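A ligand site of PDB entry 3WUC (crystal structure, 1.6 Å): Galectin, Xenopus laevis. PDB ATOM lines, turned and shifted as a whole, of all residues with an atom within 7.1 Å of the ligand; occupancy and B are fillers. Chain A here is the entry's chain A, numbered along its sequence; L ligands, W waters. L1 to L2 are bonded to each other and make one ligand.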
ATOM      1  N   MET A   3      15.953 -26.801 -20.054  1.00  0.00           N
ATOM      2  CA  MET A   3      14.944 -25.706 -19.939  1.00  0.00           C
ATOM      3  C   MET A   3      13.881 -26.124 -18.908  1.00  0.00           C
ATOM      4  O   MET A   3      13.751 -27.320 -18.608  1.00  0.00           O
ATOM      5  CB  MET A   3      14.335 -25.424 -21.298  1.00  0.00           C
ATOM      6  CG  MET A   3      13.250 -26.430 -21.724  1.00  0.00           C
ATOM      7  SD  MET A   3      12.158 -25.983 -23.088  1.00  0.00           S
ATOM      8  CE  MET A   3      11.433 -27.599 -23.330  1.00  0.00           C
ATOM      9  N   ASP A   4      13.095 -25.181 -18.367  1.00  0.00           N
ATOM     10  CA  ASP A   4      12.045 -25.543 -17.385  1.00  0.00           C
ATOM     11  C   ASP A   4      10.708 -25.979 -17.984  1.00  0.00           C
ATOM     12  O   ASP A   4       9.962 -26.716 -17.396  1.00  0.00           O
ATOM     13  CB  ASP A   4      11.727 -24.398 -16.394  1.00  0.00           C
ATOM     14  CG  ASP A   4      11.308 -23.106 -17.073  1.00  0.00           C
ATOM     15  OD1 ASP A   4      11.656 -23.003 -18.213  1.00  0.00           O
ATOM     16  OD2 ASP A   4      10.670 -22.215 -16.518  1.00  0.00           O
ATOM     17  N   MET A   5      10.366 -25.462 -19.155  1.00  0.00           N
ATOM     18  CA  MET A   5       9.078 -25.708 -19.730  1.00  0.00           C
ATOM     19  C   MET A   5       8.895 -27.172 -20.173  1.00  0.00           C
ATOM     20  O   MET A   5       9.861 -27.803 -20.486  1.00  0.00           O
ATOM     21  CB  MET A   5       8.927 -24.828 -21.025  1.00  0.00           C
ATOM     22  CG  MET A   5       8.850 -23.338 -20.764  1.00  0.00           C
ATOM     23  SD  MET A   5       8.605 -22.293 -22.262  1.00  0.00           S
ATOM     24  CE  MET A   5      10.257 -22.468 -22.956  1.00  0.00           C
ATOM     25  N   ARG A  34       5.006 -19.242 -18.458  1.00  0.00           N
ATOM     26  CA  ARG A  34       5.359 -18.824 -19.786  1.00  0.00           C
ATOM     27  C   ARG A  34       5.126 -19.992 -20.736  1.00  0.00           C
ATOM     28  O   ARG A  34       5.095 -21.140 -20.302  1.00  0.00           O
ATOM     29  CB  ARG A  34       6.800 -18.392 -19.886  1.00  0.00           C
ATOM     30  CG  ARG A  34       7.833 -19.513 -19.814  1.00  0.00           C
ATOM     31  CD  ARG A  34       9.198 -18.948 -19.409  1.00  0.00           C
ATOM     32  NE  ARG A  34      10.277 -19.972 -19.337  1.00  0.00           N
ATOM     33  CZ  ARG A  34      11.324 -19.996 -20.151  1.00  0.00           C
ATOM     34  NH1 ARG A  34      11.492 -19.204 -21.202  1.00  0.00           N
ATOM     35  NH2 ARG A  34      12.242 -20.943 -19.949  1.00  0.00           N
ATOM     36  N   ALA A  36       6.173 -21.131 -25.192  1.00  0.00           N
ATOM     37  CA  ALA A  36       6.886 -20.726 -26.351  1.00  0.00           C
ATOM     38  C   ALA A  36       6.547 -21.533 -27.567  1.00  0.00           C
ATOM     39  O   ALA A  36       6.166 -22.713 -27.451  1.00  0.00           O
ATOM     40  CB  ALA A  36       8.359 -20.968 -26.117  1.00  0.00           C
ATOM     41  N   HIS A  49      12.303 -17.712 -31.466  1.00  0.00           N
ATOM     42  CA  HIS A  49      11.796 -18.185 -30.173  1.00  0.00           C
ATOM     43  C   HIS A  49      10.843 -17.152 -29.687  1.00  0.00           C
ATOM     44  O   HIS A  49      11.185 -16.008 -29.405  1.00  0.00           O
ATOM     45  CB  HIS A  49      12.947 -18.342 -29.211  1.00  0.00           C
ATOM     46  CG  HIS A  49      12.587 -18.565 -27.781  1.00  0.00           C
ATOM     47  ND1 HIS A  49      12.089 -19.730 -27.238  1.00  0.00           N
ATOM     48  CD2 HIS A  49      12.749 -17.743 -26.689  1.00  0.00           C
ATOM     49  CE1 HIS A  49      11.978 -19.643 -25.919  1.00  0.00           C
ATOM     50  NE2 HIS A  49      12.403 -18.447 -25.565  1.00  0.00           N
ATOM     51  N   ASN A  51       8.218 -16.208 -27.031  1.00  0.00           N
ATOM     52  CA  ASN A  51       8.074 -16.632 -25.646  1.00  0.00           C
ATOM     53  C   ASN A  51       7.227 -15.721 -24.731  1.00  0.00           C
ATOM     54  O   ASN A  51       7.727 -14.854 -23.999  1.00  0.00           O
ATOM     55  CB  ASN A  51       9.460 -16.790 -25.015  1.00  0.00           C
ATOM     56  CG  ASN A  51       9.456 -17.443 -23.620  1.00  0.00           C
ATOM     57  OD1 ASN A  51      10.305 -17.043 -22.775  1.00  0.00           O
ATOM     58  ND2 ASN A  51       8.472 -18.305 -23.276  1.00  0.00           N
ATOM     59  N   ARG A  53       5.573 -14.432 -21.614  1.00  0.00           N
ATOM     60  CA  ARG A  53       5.776 -14.640 -20.209  1.00  0.00           C
ATOM     61  C   ARG A  53       4.722 -13.941 -19.402  1.00  0.00           C
ATOM     62  O   ARG A  53       4.590 -12.713 -19.421  1.00  0.00           O
ATOM     63  CB  ARG A  53       7.120 -14.073 -19.883  1.00  0.00           C
ATOM     64  CG  ARG A  53       8.280 -14.802 -20.564  1.00  0.00           C
ATOM     65  CD  ARG A  53       9.637 -14.088 -20.388  1.00  0.00           C
ATOM     66  NE  ARG A  53      10.695 -14.929 -20.978  1.00  0.00           N
ATOM     67  CZ  ARG A  53      12.011 -14.774 -20.773  1.00  0.00           C
ATOM     68  NH1 ARG A  53      12.374 -13.831 -19.965  1.00  0.00           N
ATOM     69  NH2 ARG A  53      12.857 -15.609 -21.312  1.00  0.00           N
ATOM     70  N   TYR A  56       8.179 -14.366 -15.656  1.00  0.00           N
ATOM     71  CA  TYR A  56       9.449 -15.074 -15.633  1.00  0.00           C
ATOM     72  C   TYR A  56      10.541 -14.082 -15.714  1.00  0.00           C
ATOM     73  O   TYR A  56      10.558 -13.160 -16.553  1.00  0.00           O
ATOM     74  CB  TYR A  56       9.543 -16.060 -16.842  1.00  0.00           C
ATOM     75  CG  TYR A  56      10.769 -16.946 -16.899  1.00  0.00           C
ATOM     76  CD1 TYR A  56      10.805 -18.138 -16.156  1.00  0.00           C
ATOM     77  CD2 TYR A  56      11.838 -16.615 -17.687  1.00  0.00           C
ATOM     78  CE1 TYR A  56      11.921 -18.901 -16.224  1.00  0.00           C
ATOM     79  CE2 TYR A  56      12.987 -17.417 -17.748  1.00  0.00           C
ATOM     80  CZ  TYR A  56      12.990 -18.558 -17.031  1.00  0.00           C
ATOM     81  OH  TYR A  56      14.147 -19.333 -17.095  1.00  0.00           O
ATOM     82  N   SER A  57      11.601 -14.353 -14.966  1.00  0.00           N
ATOM     83  CA  SER A  57      12.667 -13.392 -14.854  1.00  0.00           C
ATOM     84  C   SER A  57      12.133 -12.018 -14.463  1.00  0.00           C
ATOM     85  O   SER A  57      11.185 -11.957 -13.700  1.00  0.00           O
ATOM     86  CB  SER A  57      13.569 -13.366 -16.100  1.00  0.00           C
ATOM     87  OG  SER A  57      14.735 -12.541 -15.885  1.00  0.00           O
ATOM     88  N   VAL A  58      12.613 -10.954 -15.126  1.00  0.00           N
ATOM     89  CA  VAL A  58      12.113  -9.615 -14.806  1.00  0.00           C
ATOM     90  C   VAL A  58      10.833  -9.295 -15.587  1.00  0.00           C
ATOM     91  O   VAL A  58      10.321  -8.208 -15.485  1.00  0.00           O
ATOM     92  CB  VAL A  58      13.152  -8.572 -15.223  1.00  0.00           C
ATOM     93  CG1 VAL A  58      14.385  -8.704 -14.330  1.00  0.00           C
ATOM     94  CG2 VAL A  58      13.512  -8.675 -16.685  1.00  0.00           C
ATOM     95  N   ASP A  59      10.336 -10.225 -16.387  1.00  0.00           N
ATOM     96  CA  ASP A  59       9.189  -9.974 -17.255  1.00  0.00           C
ATOM     97  C   ASP A  59       7.851 -10.415 -16.734  1.00  0.00           C
ATOM     98  O   ASP A  59       7.677 -11.548 -16.295  1.00  0.00           O
ATOM     99  CB  ASP A  59       9.458 -10.662 -18.616  1.00  0.00           C
ATOM    100  CG  ASP A  59      10.762 -10.233 -19.194  1.00  0.00           C
ATOM    101  OD1 ASP A  59      11.008  -8.994 -19.353  1.00  0.00           O
ATOM    102  OD2 ASP A  59      11.586 -11.152 -19.424  1.00  0.00           O
ATOM    103  N   VAL A  64       8.813 -12.139 -24.918  1.00  0.00           N
ATOM    104  CA  VAL A  64      10.239 -12.090 -25.328  1.00  0.00           C
ATOM    105  C   VAL A  64      10.374 -12.836 -26.646  1.00  0.00           C
ATOM    106  O   VAL A  64       9.840 -13.984 -26.750  1.00  0.00           O
ATOM    107  CB  VAL A  64      11.091 -12.763 -24.235  1.00  0.00           C
ATOM    108  CG1 VAL A  64      12.498 -13.162 -24.731  1.00  0.00           C
ATOM    109  CG2 VAL A  64      11.147 -11.908 -22.983  1.00  0.00           C
ATOM    110  N   LEU A  65      11.018 -12.183 -27.584  1.00  0.00           N
ATOM    111  CA  LEU A  65      11.445 -12.853 -28.835  1.00  0.00           C
ATOM    112  C   LEU A  65      12.956 -12.981 -28.826  1.00  0.00           C
ATOM    113  O   LEU A  65      13.681 -12.030 -28.428  1.00  0.00           O
ATOM    114  CB  LEU A  65      11.040 -12.034 -30.070  1.00  0.00           C
ATOM    115  CG  LEU A  65       9.511 -11.811 -30.189  1.00  0.00           C
ATOM    116  CD1 LEU A  65       9.286 -10.899 -31.372  1.00  0.00           C
ATOM    117  CD2 LEU A  65       8.774 -13.072 -30.480  1.00  0.00           C
ATOM    118  N   ASN A  66      13.521 -14.071 -29.303  1.00  0.00           N
ATOM    119  CA  ASN A  66      14.955 -14.225 -29.440  1.00  0.00           C
ATOM    120  C   ASN A  66      15.280 -15.253 -30.536  1.00  0.00           C
ATOM    121  O   ASN A  66      14.417 -15.897 -31.081  1.00  0.00           O
ATOM    122  CB  ASN A  66      15.611 -14.573 -28.124  1.00  0.00           C
ATOM    123  CG  ASN A  66      17.029 -14.077 -28.032  1.00  0.00           C
ATOM    124  OD1 ASN A  66      17.624 -13.623 -28.999  1.00  0.00           O
ATOM    125  ND2 ASN A  66      17.580 -14.232 -26.852  1.00  0.00           N
ATOM    126  N   SER A  67      16.547 -15.333 -30.887  1.00  0.00           N
ATOM    127  CA  SER A  67      17.126 -16.304 -31.763  1.00  0.00           C
ATOM    128  C   SER A  67      18.238 -17.077 -31.013  1.00  0.00           C
ATOM    129  O   SER A  67      18.724 -16.585 -30.002  1.00  0.00           O
ATOM    130  CB  SER A  67      17.693 -15.714 -33.047  1.00  0.00           C
ATOM    131  OG  SER A  67      18.541 -14.621 -32.694  1.00  0.00           O
ATOM    132  N   TRP A  73      21.925 -18.167 -26.969  1.00  0.00           N
ATOM    133  CA  TRP A  73      20.848 -17.161 -27.159  1.00  0.00           C
ATOM    134  C   TRP A  73      21.471 -15.840 -27.642  1.00  0.00           C
ATOM    135  O   TRP A  73      22.564 -15.381 -27.164  1.00  0.00           O
ATOM    136  CB  TRP A  73      20.109 -16.940 -25.862  1.00  0.00           C
ATOM    137  CG  TRP A  73      19.242 -18.056 -25.471  1.00  0.00           C
ATOM    138  CD1 TRP A  73      19.433 -18.932 -24.418  1.00  0.00           C
ATOM    139  CD2 TRP A  73      18.063 -18.506 -26.130  1.00  0.00           C
ATOM    140  NE1 TRP A  73      18.416 -19.854 -24.366  1.00  0.00           N
ATOM    141  CE2 TRP A  73      17.569 -19.618 -25.413  1.00  0.00           C
ATOM    142  CE3 TRP A  73      17.369 -18.059 -27.253  1.00  0.00           C
ATOM    143  CZ2 TRP A  73      16.397 -20.258 -25.765  1.00  0.00           C
ATOM    144  CZ3 TRP A  73      16.235 -18.758 -27.621  1.00  0.00           C
ATOM    145  CH2 TRP A  73      15.752 -19.808 -26.869  1.00  0.00           C
ATOM    146  N   ASP A  74      20.808 -15.187 -28.565  1.00  0.00           N
ATOM    147  CA  ASP A  74      21.133 -13.819 -29.008  1.00  0.00           C
ATOM    148  C   ASP A  74      20.505 -12.773 -28.030  1.00  0.00           C
ATOM    149  O   ASP A  74      20.229 -13.090 -26.870  1.00  0.00           O
ATOM    150  CB  ASP A  74      20.753 -13.661 -30.473  1.00  0.00           C
ATOM    151  CG  ASP A  74      21.554 -14.544 -31.397  1.00  0.00           C
ATOM    152  OD1 ASP A  74      22.784 -14.732 -31.166  1.00  0.00           O
ATOM    153  OD2 ASP A  74      20.990 -15.172 -32.332  1.00  0.00           O
ATOM    154  N   ILE A  75      20.355 -11.534 -28.485  1.00  0.00           N
ATOM    155  CA  ILE A  75      19.811 -10.498 -27.652  1.00  0.00           C
ATOM    156  C   ILE A  75      18.281 -10.463 -27.722  1.00  0.00           C
ATOM    157  O   ILE A  75      17.720 -10.387 -28.799  1.00  0.00           O
ATOM    158  CB  ILE A  75      20.434  -9.128 -28.007  1.00  0.00           C
ATOM    159  CG1 ILE A  75      21.963  -9.194 -27.673  1.00  0.00           C
ATOM    160  CG2 ILE A  75      19.821  -8.052 -27.148  1.00  0.00           C
ATOM    161  CD1 ILE A  75      22.792  -8.659 -28.767  1.00  0.00           C
ATOM    162  N   GLU A  76      17.632 -10.537 -26.571  1.00  0.00           N
ATOM    163  CA  GLU A  76      16.171 -10.510 -26.496  1.00  0.00           C
ATOM    164  C   GLU A  76      15.555  -9.228 -26.990  1.00  0.00           C
ATOM    165  O   GLU A  76      16.079  -8.122 -26.785  1.00  0.00           O
ATOM    166  CB  GLU A  76      15.672 -10.729 -25.080  1.00  0.00           C
ATOM    167  CG  GLU A  76      15.997 -12.055 -24.537  1.00  0.00           C
ATOM    168  CD  GLU A  76      15.728 -12.203 -23.068  1.00  0.00           C
ATOM    169  OE1 GLU A  76      15.337 -11.233 -22.363  1.00  0.00           O
ATOM    170  OE2 GLU A  76      15.934 -13.318 -22.617  1.00  0.00           O
ATOM    171  N   LYS A  77      14.482  -9.327 -27.740  1.00  0.00           N
ATOM    172  CA  LYS A  77      13.566  -8.210 -28.054  1.00  0.00           C
ATOM    173  C   LYS A  77      12.244  -8.395 -27.321  1.00  0.00           C
ATOM    174  O   LYS A  77      11.754  -9.547 -27.144  1.00  0.00           O
ATOM    175  CB  LYS A  77      13.316  -8.209 -29.547  1.00  0.00           C
ATOM    176  CG  LYS A  77      14.453  -7.803 -30.447  1.00  0.00           C
ATOM    177  CD  LYS A  77      14.324  -6.282 -30.765  1.00  0.00           C
ATOM    178  CE  LYS A  77      15.451  -5.723 -31.606  1.00  0.00           C
ATOM    179  NZ  LYS A  77      15.420  -4.222 -31.851  1.00  0.00           N
ATOM    180  N   LYS A  78      11.661  -7.309 -26.803  1.00  0.00           N
ATOM    181  CA  LYS A  78      10.503  -7.529 -25.953  1.00  0.00           C
ATOM    182  C   LYS A  78       9.328  -6.623 -26.434  1.00  0.00           C
ATOM    183  O   LYS A  78       9.568  -5.473 -26.860  1.00  0.00           O
ATOM    184  CB  LYS A  78      10.781  -7.096 -24.554  1.00  0.00           C
ATOM    185  CG  LYS A  78      11.957  -7.819 -23.894  1.00  0.00           C
ATOM    186  CD  LYS A  78      12.050  -7.587 -22.420  1.00  0.00           C
ATOM    187  CE  LYS A  78      13.259  -8.309 -21.834  1.00  0.00           C
ATOM    188  NZ  LYS A  78      13.257  -8.013 -20.388  1.00  0.00           N
HETATM  189  C1  LIG L   1      18.118 -13.424 -18.063  1.00  0.00           C
HETATM  190  C2  LIG L   1      16.850 -13.005 -18.865  1.00  0.00           C
HETATM  191  C3  LIG L   1      16.073 -14.300 -19.162  1.00  0.00           C
HETATM  192  C4  LIG L   1      16.922 -15.468 -19.668  1.00  0.00           C
HETATM  193  C5  LIG L   1      17.891 -15.798 -18.543  1.00  0.00           C
HETATM  194  C6  LIG L   1      18.682 -17.070 -18.748  1.00  0.00           C
HETATM  195  O1  LIG L   1      17.492 -13.748 -16.877  1.00  0.00           O
HETATM  196  O2  LIG L   1      16.017 -12.058 -18.241  1.00  0.00           O
HETATM  197  O3  LIG L   1      15.179 -13.981 -20.210  1.00  0.00           O
HETATM  198  O4  LIG L   1      16.067 -16.642 -19.770  1.00  0.00           O
HETATM  199  O5  LIG L   1      18.717 -14.678 -18.305  1.00  0.00           O
HETATM  200  O6  LIG L   1      19.616 -16.716 -19.725  1.00  0.00           O
HETATM  201  C1  LG2 L   2      16.191 -17.429 -20.933  1.00  0.00           C
HETATM  202  C2  LG2 L   2      15.337 -18.700 -20.761  1.00  0.00           C
HETATM  203  C3  LG2 L   2      15.159 -19.424 -22.094  1.00  0.00           C
HETATM  204  C4  LG2 L   2      14.774 -18.440 -23.231  1.00  0.00           C
HETATM  205  C5  LG2 L   2      15.730 -17.267 -23.231  1.00  0.00           C
HETATM  206  C6  LG2 L   2      15.388 -16.253 -24.322  1.00  0.00           C
HETATM  207  O1  LG2 L   2      15.832 -19.566 -19.706  1.00  0.00           O
HETATM  208  O2  LG2 L   2      14.293 -20.539 -21.958  1.00  0.00           O
HETATM  209  O3  LG2 L   2      13.401 -18.056 -23.077  1.00  0.00           O
HETATM  210  O4  LG2 L   2      15.669 -16.619 -21.961  1.00  0.00           O
HETATM  211  O5  LG2 L   2      16.326 -15.205 -24.405  1.00  0.00           O
HETATM  212  O   HOH W   1      17.383  -9.733 -17.601  1.00  0.00           O
HETATM  213  O   HOH W   2      14.348 -10.851 -19.849  1.00  0.00           O
HETATM  214  O   HOH W   3      18.827 -15.297 -23.008  1.00  0.00           O
HETATM  215  O   HOH W   4      18.489 -20.532 -20.231  1.00  0.00           O
HETATM  216  O   HOH W   5      15.643 -22.348 -19.817  1.00  0.00           O
HETATM  217  O   HOH W   6      19.083 -12.944 -14.709  1.00  0.00           O
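The guanidinium group (NH2) of Arg 34 sits at hydrogen-bond distance from an oxygen (O2) of LG2 L2 (2.9 Å).
An oxygen (O3) of LIG L1 sits at hydrogen-bond distance from the side-chain carboxylate of Glu 76 (2.6 Å).
The side-chain hydroxyl of Ser 57 is in hydrogen-bond range of an oxygen (O2) of LIG L1 (2.7 Å).
The guanidinium group (NH1) of Arg 53 lies within hydrogen-bond range of an oxygen (O3) of LIG L1, 2.8 Å away.
OH of Tyr 56 sits at hydrogen-bond distance from O1 of LG2 L2, 3.1 Å away.
An oxygen (O5) of LG2 L2 is in hydrogen-bond range of the side-chain amide nitrogen (ND2) of Asn 66 (2.9 Å).
The side-chain amide oxygen of Asn 51 is in hydrogen-bond range of an oxygen (O3) of LG2 L2 (3.3 Å).
NE2 of His 49 lies within hydrogen-bond range of O3 of LG2 L2, at 2.7 Å.
NH1 of Arg 34 lies within hydrogen-bond range of OD1 of Asn 51, 2.9 Å away.
OD2 of Asp 59 is in salt-bridge range of NH1 of Arg 53, at 2.8 Å.
NE of Arg 53 is in hydrogen-bond range of OD1 of Asn 51.
The backbone carbonyl oxygen of Ile 75 sits close to the side-chain amide oxygen of Asn 66 (3.2 Å).
N of His 49 lies within hydrogen-bond range of O of Asn 66 (2.8 Å).
The backbone carbonyl oxygen of Asp 74 is in hydrogen-bond range of the side-chain amide nitrogen of Asn 66.
NH2 of Arg 34 lies within salt-bridge range of OD1 of Asp 4 (2.8 Å).
The backbone NH (N) of Asn 51 lies within hydrogen-bond range of the backbone carbonyl oxygen (O) of Val 64 (2.8 Å).
Trp 73 touches the ligand.
Of the 22 residues printed, 9 come within 4 Å of the ligand.
Water W2 lies within hydrogen-bond range of an oxygen (O2) of LIG L1 (2.6 Å), the side-chain carboxylate of Glu 76 (2.7 Å), the side-chain carboxylate of Asp 59 (2.8 Å) and the side-chain amino group of Lys 78 (3.1 Å).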
